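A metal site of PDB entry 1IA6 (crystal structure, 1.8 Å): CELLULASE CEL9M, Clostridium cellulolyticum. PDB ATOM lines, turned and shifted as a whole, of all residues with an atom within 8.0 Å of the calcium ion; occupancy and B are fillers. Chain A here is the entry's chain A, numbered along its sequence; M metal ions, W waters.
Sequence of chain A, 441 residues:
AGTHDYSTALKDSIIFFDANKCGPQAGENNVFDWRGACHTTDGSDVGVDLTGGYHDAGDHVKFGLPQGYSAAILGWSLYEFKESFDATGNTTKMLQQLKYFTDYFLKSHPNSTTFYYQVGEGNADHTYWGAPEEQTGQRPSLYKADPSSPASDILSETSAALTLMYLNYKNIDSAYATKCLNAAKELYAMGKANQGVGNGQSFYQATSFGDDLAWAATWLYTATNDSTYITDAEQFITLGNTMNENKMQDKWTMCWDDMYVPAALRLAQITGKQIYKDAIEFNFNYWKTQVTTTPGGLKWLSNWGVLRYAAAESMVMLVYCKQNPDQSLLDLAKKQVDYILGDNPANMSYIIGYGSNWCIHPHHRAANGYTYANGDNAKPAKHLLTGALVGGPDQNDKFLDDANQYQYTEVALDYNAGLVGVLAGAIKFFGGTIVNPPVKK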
ATOM      1  N   LEU A  65       4.691   9.404  -5.248  1.00  0.00           N
ATOM      2  CA  LEU A  65       4.019   8.951  -4.033  1.00  0.00           C
ATOM      3  C   LEU A  65       3.216  10.043  -3.337  1.00  0.00           C
ATOM      4  O   LEU A  65       2.021   9.866  -3.095  1.00  0.00           O
ATOM      5  CB  LEU A  65       5.024   8.305  -3.064  1.00  0.00           C
ATOM      6  CG  LEU A  65       4.417   7.609  -1.831  1.00  0.00           C
ATOM      7  CD1 LEU A  65       3.229   6.739  -2.238  1.00  0.00           C
ATOM      8  CD2 LEU A  65       5.493   6.773  -1.151  1.00  0.00           C
ATOM      9  N   SER A 152       4.405  -0.517  -6.389  1.00  0.00           N
ATOM     10  CA  SER A 152       3.132  -0.885  -5.779  1.00  0.00           C
ATOM     11  C   SER A 152       2.479   0.173  -4.904  1.00  0.00           C
ATOM     12  O   SER A 152       1.256   0.335  -4.930  1.00  0.00           O
ATOM     13  CB  SER A 152       3.284  -2.171  -4.968  1.00  0.00           C
ATOM     14  OG  SER A 152       3.795  -3.218  -5.787  1.00  0.00           O
ATOM     15  N   ASP A 153       3.281   0.883  -4.118  1.00  0.00           N
ATOM     16  CA  ASP A 153       2.730   1.917  -3.246  1.00  0.00           C
ATOM     17  C   ASP A 153       2.219   3.109  -4.043  1.00  0.00           C
ATOM     18  O   ASP A 153       1.106   3.593  -3.810  1.00  0.00           O
ATOM     19  CB  ASP A 153       3.752   2.338  -2.179  1.00  0.00           C
ATOM     20  CG  ASP A 153       5.095   2.759  -2.775  1.00  0.00           C
ATOM     21  OD1 ASP A 153       5.400   2.391  -3.926  1.00  0.00           O
ATOM     22  OD2 ASP A 153       5.870   3.433  -2.065  1.00  0.00           O
ATOM     23  N   ILE A 154       3.026   3.579  -4.994  1.00  0.00           N
ATOM     24  CA  ILE A 154       2.643   4.707  -5.828  1.00  0.00           C
ATOM     25  C   ILE A 154       1.431   4.371  -6.684  1.00  0.00           C
ATOM     26  O   ILE A 154       0.468   5.133  -6.756  1.00  0.00           O
ATOM     27  CB  ILE A 154       3.827   5.136  -6.726  1.00  0.00           C
ATOM     28  CG1 ILE A 154       4.974   5.642  -5.842  1.00  0.00           C
ATOM     29  CG2 ILE A 154       3.380   6.220  -7.723  1.00  0.00           C
ATOM     30  CD1 ILE A 154       6.178   6.140  -6.619  1.00  0.00           C
ATOM     31  N   GLU A 157      -1.777   4.226  -4.460  1.00  0.00           N
ATOM     32  CA  GLU A 157      -2.320   5.503  -4.012  1.00  0.00           C
ATOM     33  C   GLU A 157      -2.982   6.205  -5.192  1.00  0.00           C
ATOM     34  O   GLU A 157      -4.019   6.853  -5.029  1.00  0.00           O
ATOM     35  CB  GLU A 157      -1.228   6.383  -3.408  1.00  0.00           C
ATOM     36  CG  GLU A 157      -0.775   5.937  -2.014  1.00  0.00           C
ATOM     37  CD  GLU A 157      -1.936   5.744  -1.054  1.00  0.00           C
ATOM     38  OE1 GLU A 157      -2.886   6.554  -1.081  1.00  0.00           O
ATOM     39  OE2 GLU A 157      -1.890   4.792  -0.251  1.00  0.00           O
ATOM     40  N   VAL A 197       8.255  -1.316  -3.565  1.00  0.00           N
ATOM     41  CA  VAL A 197       7.996   0.115  -3.494  1.00  0.00           C
ATOM     42  C   VAL A 197       8.606   0.867  -4.681  1.00  0.00           C
ATOM     43  O   VAL A 197       9.600   0.414  -5.265  1.00  0.00           O
ATOM     44  CB  VAL A 197       8.561   0.745  -2.190  1.00  0.00           C
ATOM     45  CG1 VAL A 197       7.868   0.121  -0.986  1.00  0.00           C
ATOM     46  CG2 VAL A 197      10.069   0.535  -2.111  1.00  0.00           C
ATOM     47  N   ALA A 206      10.373   5.306   0.363  1.00  0.00           N
ATOM     48  CA  ALA A 206       9.259   4.502   0.848  1.00  0.00           C
ATOM     49  C   ALA A 206       9.709   3.224   1.530  1.00  0.00           C
ATOM     50  O   ALA A 206      10.783   2.687   1.234  1.00  0.00           O
ATOM     51  CB  ALA A 206       8.325   4.176  -0.305  1.00  0.00           C
ATOM     52  N   THR A 207       8.888   2.724   2.444  1.00  0.00           N
ATOM     53  CA  THR A 207       9.214   1.516   3.200  1.00  0.00           C
ATOM     54  C   THR A 207       8.147   0.438   3.178  1.00  0.00           C
ATOM     55  O   THR A 207       8.409  -0.685   3.616  1.00  0.00           O
ATOM     56  CB  THR A 207       9.481   1.863   4.669  1.00  0.00           C
ATOM     57  OG1 THR A 207       8.280   2.358   5.277  1.00  0.00           O
ATOM     58  CG2 THR A 207      10.571   2.925   4.787  1.00  0.00           C
ATOM     59  N   SER A 208       6.960   0.745   2.680  1.00  0.00           N
ATOM     60  CA  SER A 208       5.880  -0.237   2.686  1.00  0.00           C
ATOM     61  C   SER A 208       4.913  -0.092   1.520  1.00  0.00           C
ATOM     62  O   SER A 208       4.652   1.021   1.077  1.00  0.00           O
ATOM     63  CB  SER A 208       5.088  -0.091   3.982  1.00  0.00           C
ATOM     64  OG  SER A 208       4.525   1.216   4.043  1.00  0.00           O
ATOM     65  N   PHE A 209       4.374  -1.211   1.049  1.00  0.00           N
ATOM     66  CA  PHE A 209       3.403  -1.164  -0.040  1.00  0.00           C
ATOM     67  C   PHE A 209       2.147  -1.980   0.270  1.00  0.00           C
ATOM     68  O   PHE A 209       1.107  -1.788  -0.371  1.00  0.00           O
ATOM     69  CB  PHE A 209       4.042  -1.613  -1.362  1.00  0.00           C
ATOM     70  CG  PHE A 209       4.484  -3.044  -1.376  1.00  0.00           C
ATOM     71  CD1 PHE A 209       3.567  -4.073  -1.548  1.00  0.00           C
ATOM     72  CD2 PHE A 209       5.832  -3.366  -1.209  1.00  0.00           C
ATOM     73  CE1 PHE A 209       3.980  -5.397  -1.565  1.00  0.00           C
ATOM     74  CE2 PHE A 209       6.255  -4.690  -1.225  1.00  0.00           C
ATOM     75  CZ  PHE A 209       5.328  -5.710  -1.394  1.00  0.00           C
ATOM     76  N   GLY A 210       2.236  -2.879   1.236  1.00  0.00           N
ATOM     77  CA  GLY A 210       1.083  -3.699   1.597  1.00  0.00           C
ATOM     78  C   GLY A 210      -0.071  -2.836   2.085  1.00  0.00           C
ATOM     79  O   GLY A 210      -1.243  -3.140   1.857  1.00  0.00           O
ATOM     80  N   ASP A 211       0.265  -1.758   2.777  1.00  0.00           N
ATOM     81  CA  ASP A 211      -0.731  -0.829   3.289  1.00  0.00           C
ATOM     82  C   ASP A 211      -1.458  -0.161   2.127  1.00  0.00           C
ATOM     83  O   ASP A 211      -2.686  -0.042   2.126  1.00  0.00           O
ATOM     84  CB  ASP A 211      -0.056   0.217   4.185  1.00  0.00           C
ATOM     85  CG  ASP A 211       1.131   0.910   3.511  1.00  0.00           C
ATOM     86  OD1 ASP A 211       1.926   0.223   2.833  1.00  0.00           O
ATOM     87  OD2 ASP A 211       1.279   2.140   3.681  1.00  0.00           O
ATOM     88  N   ASP A 212      -0.701   0.285   1.123  1.00  0.00           N
ATOM     89  CA  ASP A 212      -1.287   0.950  -0.036  1.00  0.00           C
ATOM     90  C   ASP A 212      -2.154   0.006  -0.868  1.00  0.00           C
ATOM     91  O   ASP A 212      -3.251   0.378  -1.299  1.00  0.00           O
ATOM     92  CB  ASP A 212      -0.162   1.546  -0.874  1.00  0.00           C
ATOM     93  CG  ASP A 212       0.680   2.511  -0.070  1.00  0.00           C
ATOM     94  OD1 ASP A 212       0.249   3.663   0.147  1.00  0.00           O
ATOM     95  OD2 ASP A 212       1.771   2.105   0.389  1.00  0.00           O
ATOM     96  N   LEU A 213      -1.683  -1.219  -1.087  1.00  0.00           N
ATOM     97  CA  LEU A 213      -2.471  -2.184  -1.858  1.00  0.00           C
ATOM     98  C   LEU A 213      -3.807  -2.456  -1.175  1.00  0.00           C
ATOM     99  O   LEU A 213      -4.847  -2.516  -1.836  1.00  0.00           O
ATOM    100  CB  LEU A 213      -1.707  -3.502  -2.018  1.00  0.00           C
ATOM    101  CG  LEU A 213      -0.611  -3.542  -3.080  1.00  0.00           C
ATOM    102  CD1 LEU A 213       0.190  -4.834  -2.934  1.00  0.00           C
ATOM    103  CD2 LEU A 213      -1.232  -3.455  -4.472  1.00  0.00           C
ATOM    104  N   LYS A 247       2.469  -3.951  12.084  1.00  0.00           N
ATOM    105  CA  LYS A 247       1.774  -2.740  11.680  1.00  0.00           C
ATOM    106  C   LYS A 247       0.327  -2.672  12.158  1.00  0.00           C
ATOM    107  O   LYS A 247      -0.390  -1.714  11.862  1.00  0.00           O
ATOM    108  CB  LYS A 247       1.809  -2.595  10.147  1.00  0.00           C
ATOM    109  CG  LYS A 247       3.112  -2.081   9.606  1.00  0.00           C
ATOM    110  CD  LYS A 247       3.378  -0.683  10.147  1.00  0.00           C
ATOM    111  CE  LYS A 247       4.648  -0.080   9.571  1.00  0.00           C
ATOM    112  NZ  LYS A 247       4.820   1.332  10.012  1.00  0.00           N
ATOM    113  N   CYS A 255       0.213   9.049   6.577  1.00  0.00           N
ATOM    114  CA  CYS A 255       1.119   9.934   5.845  1.00  0.00           C
ATOM    115  C   CYS A 255       1.471   9.250   4.523  1.00  0.00           C
ATOM    116  O   CYS A 255       1.092   8.106   4.292  1.00  0.00           O
ATOM    117  CB  CYS A 255       2.387  10.245   6.667  1.00  0.00           C
ATOM    118  SG  CYS A 255       3.391   8.829   7.140  1.00  0.00           S
ATOM    119  N   TRP A 256       2.203   9.956   3.671  1.00  0.00           N
ATOM    120  CA  TRP A 256       2.525   9.408   2.357  1.00  0.00           C
ATOM    121  C   TRP A 256       3.159   8.017   2.351  1.00  0.00           C
ATOM    122  O   TRP A 256       2.976   7.264   1.397  1.00  0.00           O
ATOM    123  CB  TRP A 256       3.413  10.383   1.561  1.00  0.00           C
ATOM    124  CG  TRP A 256       4.703  10.759   2.206  1.00  0.00           C
ATOM    125  CD1 TRP A 256       4.936  11.833   3.021  1.00  0.00           C
ATOM    126  CD2 TRP A 256       5.938  10.044   2.128  1.00  0.00           C
ATOM    127  NE1 TRP A 256       6.252  11.828   3.440  1.00  0.00           N
ATOM    128  CE2 TRP A 256       6.884  10.745   2.904  1.00  0.00           C
ATOM    129  CE3 TRP A 256       6.349   8.873   1.458  1.00  0.00           C
ATOM    130  CZ2 TRP A 256       8.215  10.314   3.044  1.00  0.00           C
ATOM    131  CZ3 TRP A 256       7.659   8.439   1.603  1.00  0.00           C
ATOM    132  CH2 TRP A 256       8.583   9.168   2.387  1.00  0.00           C
ATOM    133  N   ASP A 257       3.900   7.668   3.400  1.00  0.00           N
ATOM    134  CA  ASP A 257       4.556   6.365   3.447  1.00  0.00           C
ATOM    135  C   ASP A 257       3.827   5.297   4.255  1.00  0.00           C
ATOM    136  O   ASP A 257       3.990   4.099   4.001  1.00  0.00           O
ATOM    137  CB  ASP A 257       5.978   6.518   4.021  1.00  0.00           C
ATOM    138  CG  ASP A 257       6.788   5.231   3.949  1.00  0.00           C
ATOM    139  OD1 ASP A 257       6.790   4.593   2.879  1.00  0.00           O
ATOM    140  OD2 ASP A 257       7.424   4.860   4.957  1.00  0.00           O
ATOM    141  N   ASP A 258       3.019   5.723   5.215  1.00  0.00           N
ATOM    142  CA  ASP A 258       2.292   4.784   6.079  1.00  0.00           C
ATOM    143  C   ASP A 258       0.782   4.946   6.011  1.00  0.00           C
ATOM    144  O   ASP A 258       0.221   5.905   6.540  1.00  0.00           O
ATOM    145  CB  ASP A 258       2.795   4.959   7.528  1.00  0.00           C
ATOM    146  CG  ASP A 258       2.086   4.044   8.516  1.00  0.00           C
ATOM    147  OD1 ASP A 258       1.409   3.094   8.092  1.00  0.00           O
ATOM    148  OD2 ASP A 258       2.226   4.294   9.732  1.00  0.00           O
ATOM    149  N   MET A 259       0.116   3.994   5.356  1.00  0.00           N
ATOM    150  CA  MET A 259      -1.332   4.038   5.216  1.00  0.00           C
ATOM    151  C   MET A 259      -1.995   2.869   5.937  1.00  0.00           C
ATOM    152  O   MET A 259      -3.146   2.538   5.647  1.00  0.00           O
ATOM    153  CB  MET A 259      -1.726   4.034   3.738  1.00  0.00           C
ATOM    154  CG  MET A 259      -1.447   5.351   3.020  1.00  0.00           C
ATOM    155  SD  MET A 259      -2.455   6.692   3.686  1.00  0.00           S
ATOM    156  CE  MET A 259      -4.004   6.382   2.845  1.00  0.00           C
ATOM    157  N   TYR A 260      -1.289   2.259   6.877  1.00  0.00           N
ATOM    158  CA  TYR A 260      -1.834   1.121   7.622  1.00  0.00           C
ATOM    159  C   TYR A 260      -3.060   1.461   8.468  1.00  0.00           C
ATOM    160  O   TYR A 260      -3.972   0.645   8.566  1.00  0.00           O
ATOM    161  CB  TYR A 260      -0.751   0.494   8.504  1.00  0.00           C
ATOM    162  CG  TYR A 260       0.191  -0.391   7.724  1.00  0.00           C
ATOM    163  CD1 TYR A 260      -0.230  -1.650   7.270  1.00  0.00           C
ATOM    164  CD2 TYR A 260       1.476   0.025   7.391  1.00  0.00           C
ATOM    165  CE1 TYR A 260       0.600  -2.446   6.496  1.00  0.00           C
ATOM    166  CE2 TYR A 260       2.317  -0.772   6.620  1.00  0.00           C
ATOM    167  CZ  TYR A 260       1.872  -2.007   6.182  1.00  0.00           C
ATOM    168  OH  TYR A 260       2.694  -2.781   5.406  1.00  0.00           O
HETATM  169 CA    CA M   1       3.215   2.612   2.223  1.00  0.00          CA
HETATM  170  O   HOH W   1       4.866   3.829   0.989  1.00  0.00           O
HETATM  171  O   HOH W   2       2.091   4.721   1.840  1.00  0.00           O
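OE2 of Glu 157 lies close to OD1 of Asp 212.
The side-chain hydroxyl (OG1) of Thr 207 lies within hydrogen-bond range of the side-chain carboxylate (OD2) of Asp 257, at 2.7 Å.
The side-chain carboxylate (OD1) of Asp 211 lies close to the backbone NH (N) of Phe 209, at 3.4 Å.
OD2 of Asp 211 sits close to N of Met 259.
Of the 21 residues printed, 4 come within 4 Å of the calcium ion.
Along chain A the residues within 4 Å of the calcium ion span positions 208 to 257.
The calcium ion is bound by OD2 of Asp 212 (2.4 Å), water W1 (2.4 Å), water W2 (2.4 Å), O of Ser 208 (2.4 Å), O of Asp 257 (2.4 Å), OD2 of Asp 211 (2.5 Å), OG of Ser 208 (2.6 Å) and OD1 of Asp 211 (2.8 Å).
The calcium ion has eight donor atoms within binding distance.
Water W1 lies within hydrogen-bond range of OD1 of Asp 257 and OD2 of Asp 153.
Water W2 bridges OD1 of Asp 212 and O of Trp 256.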
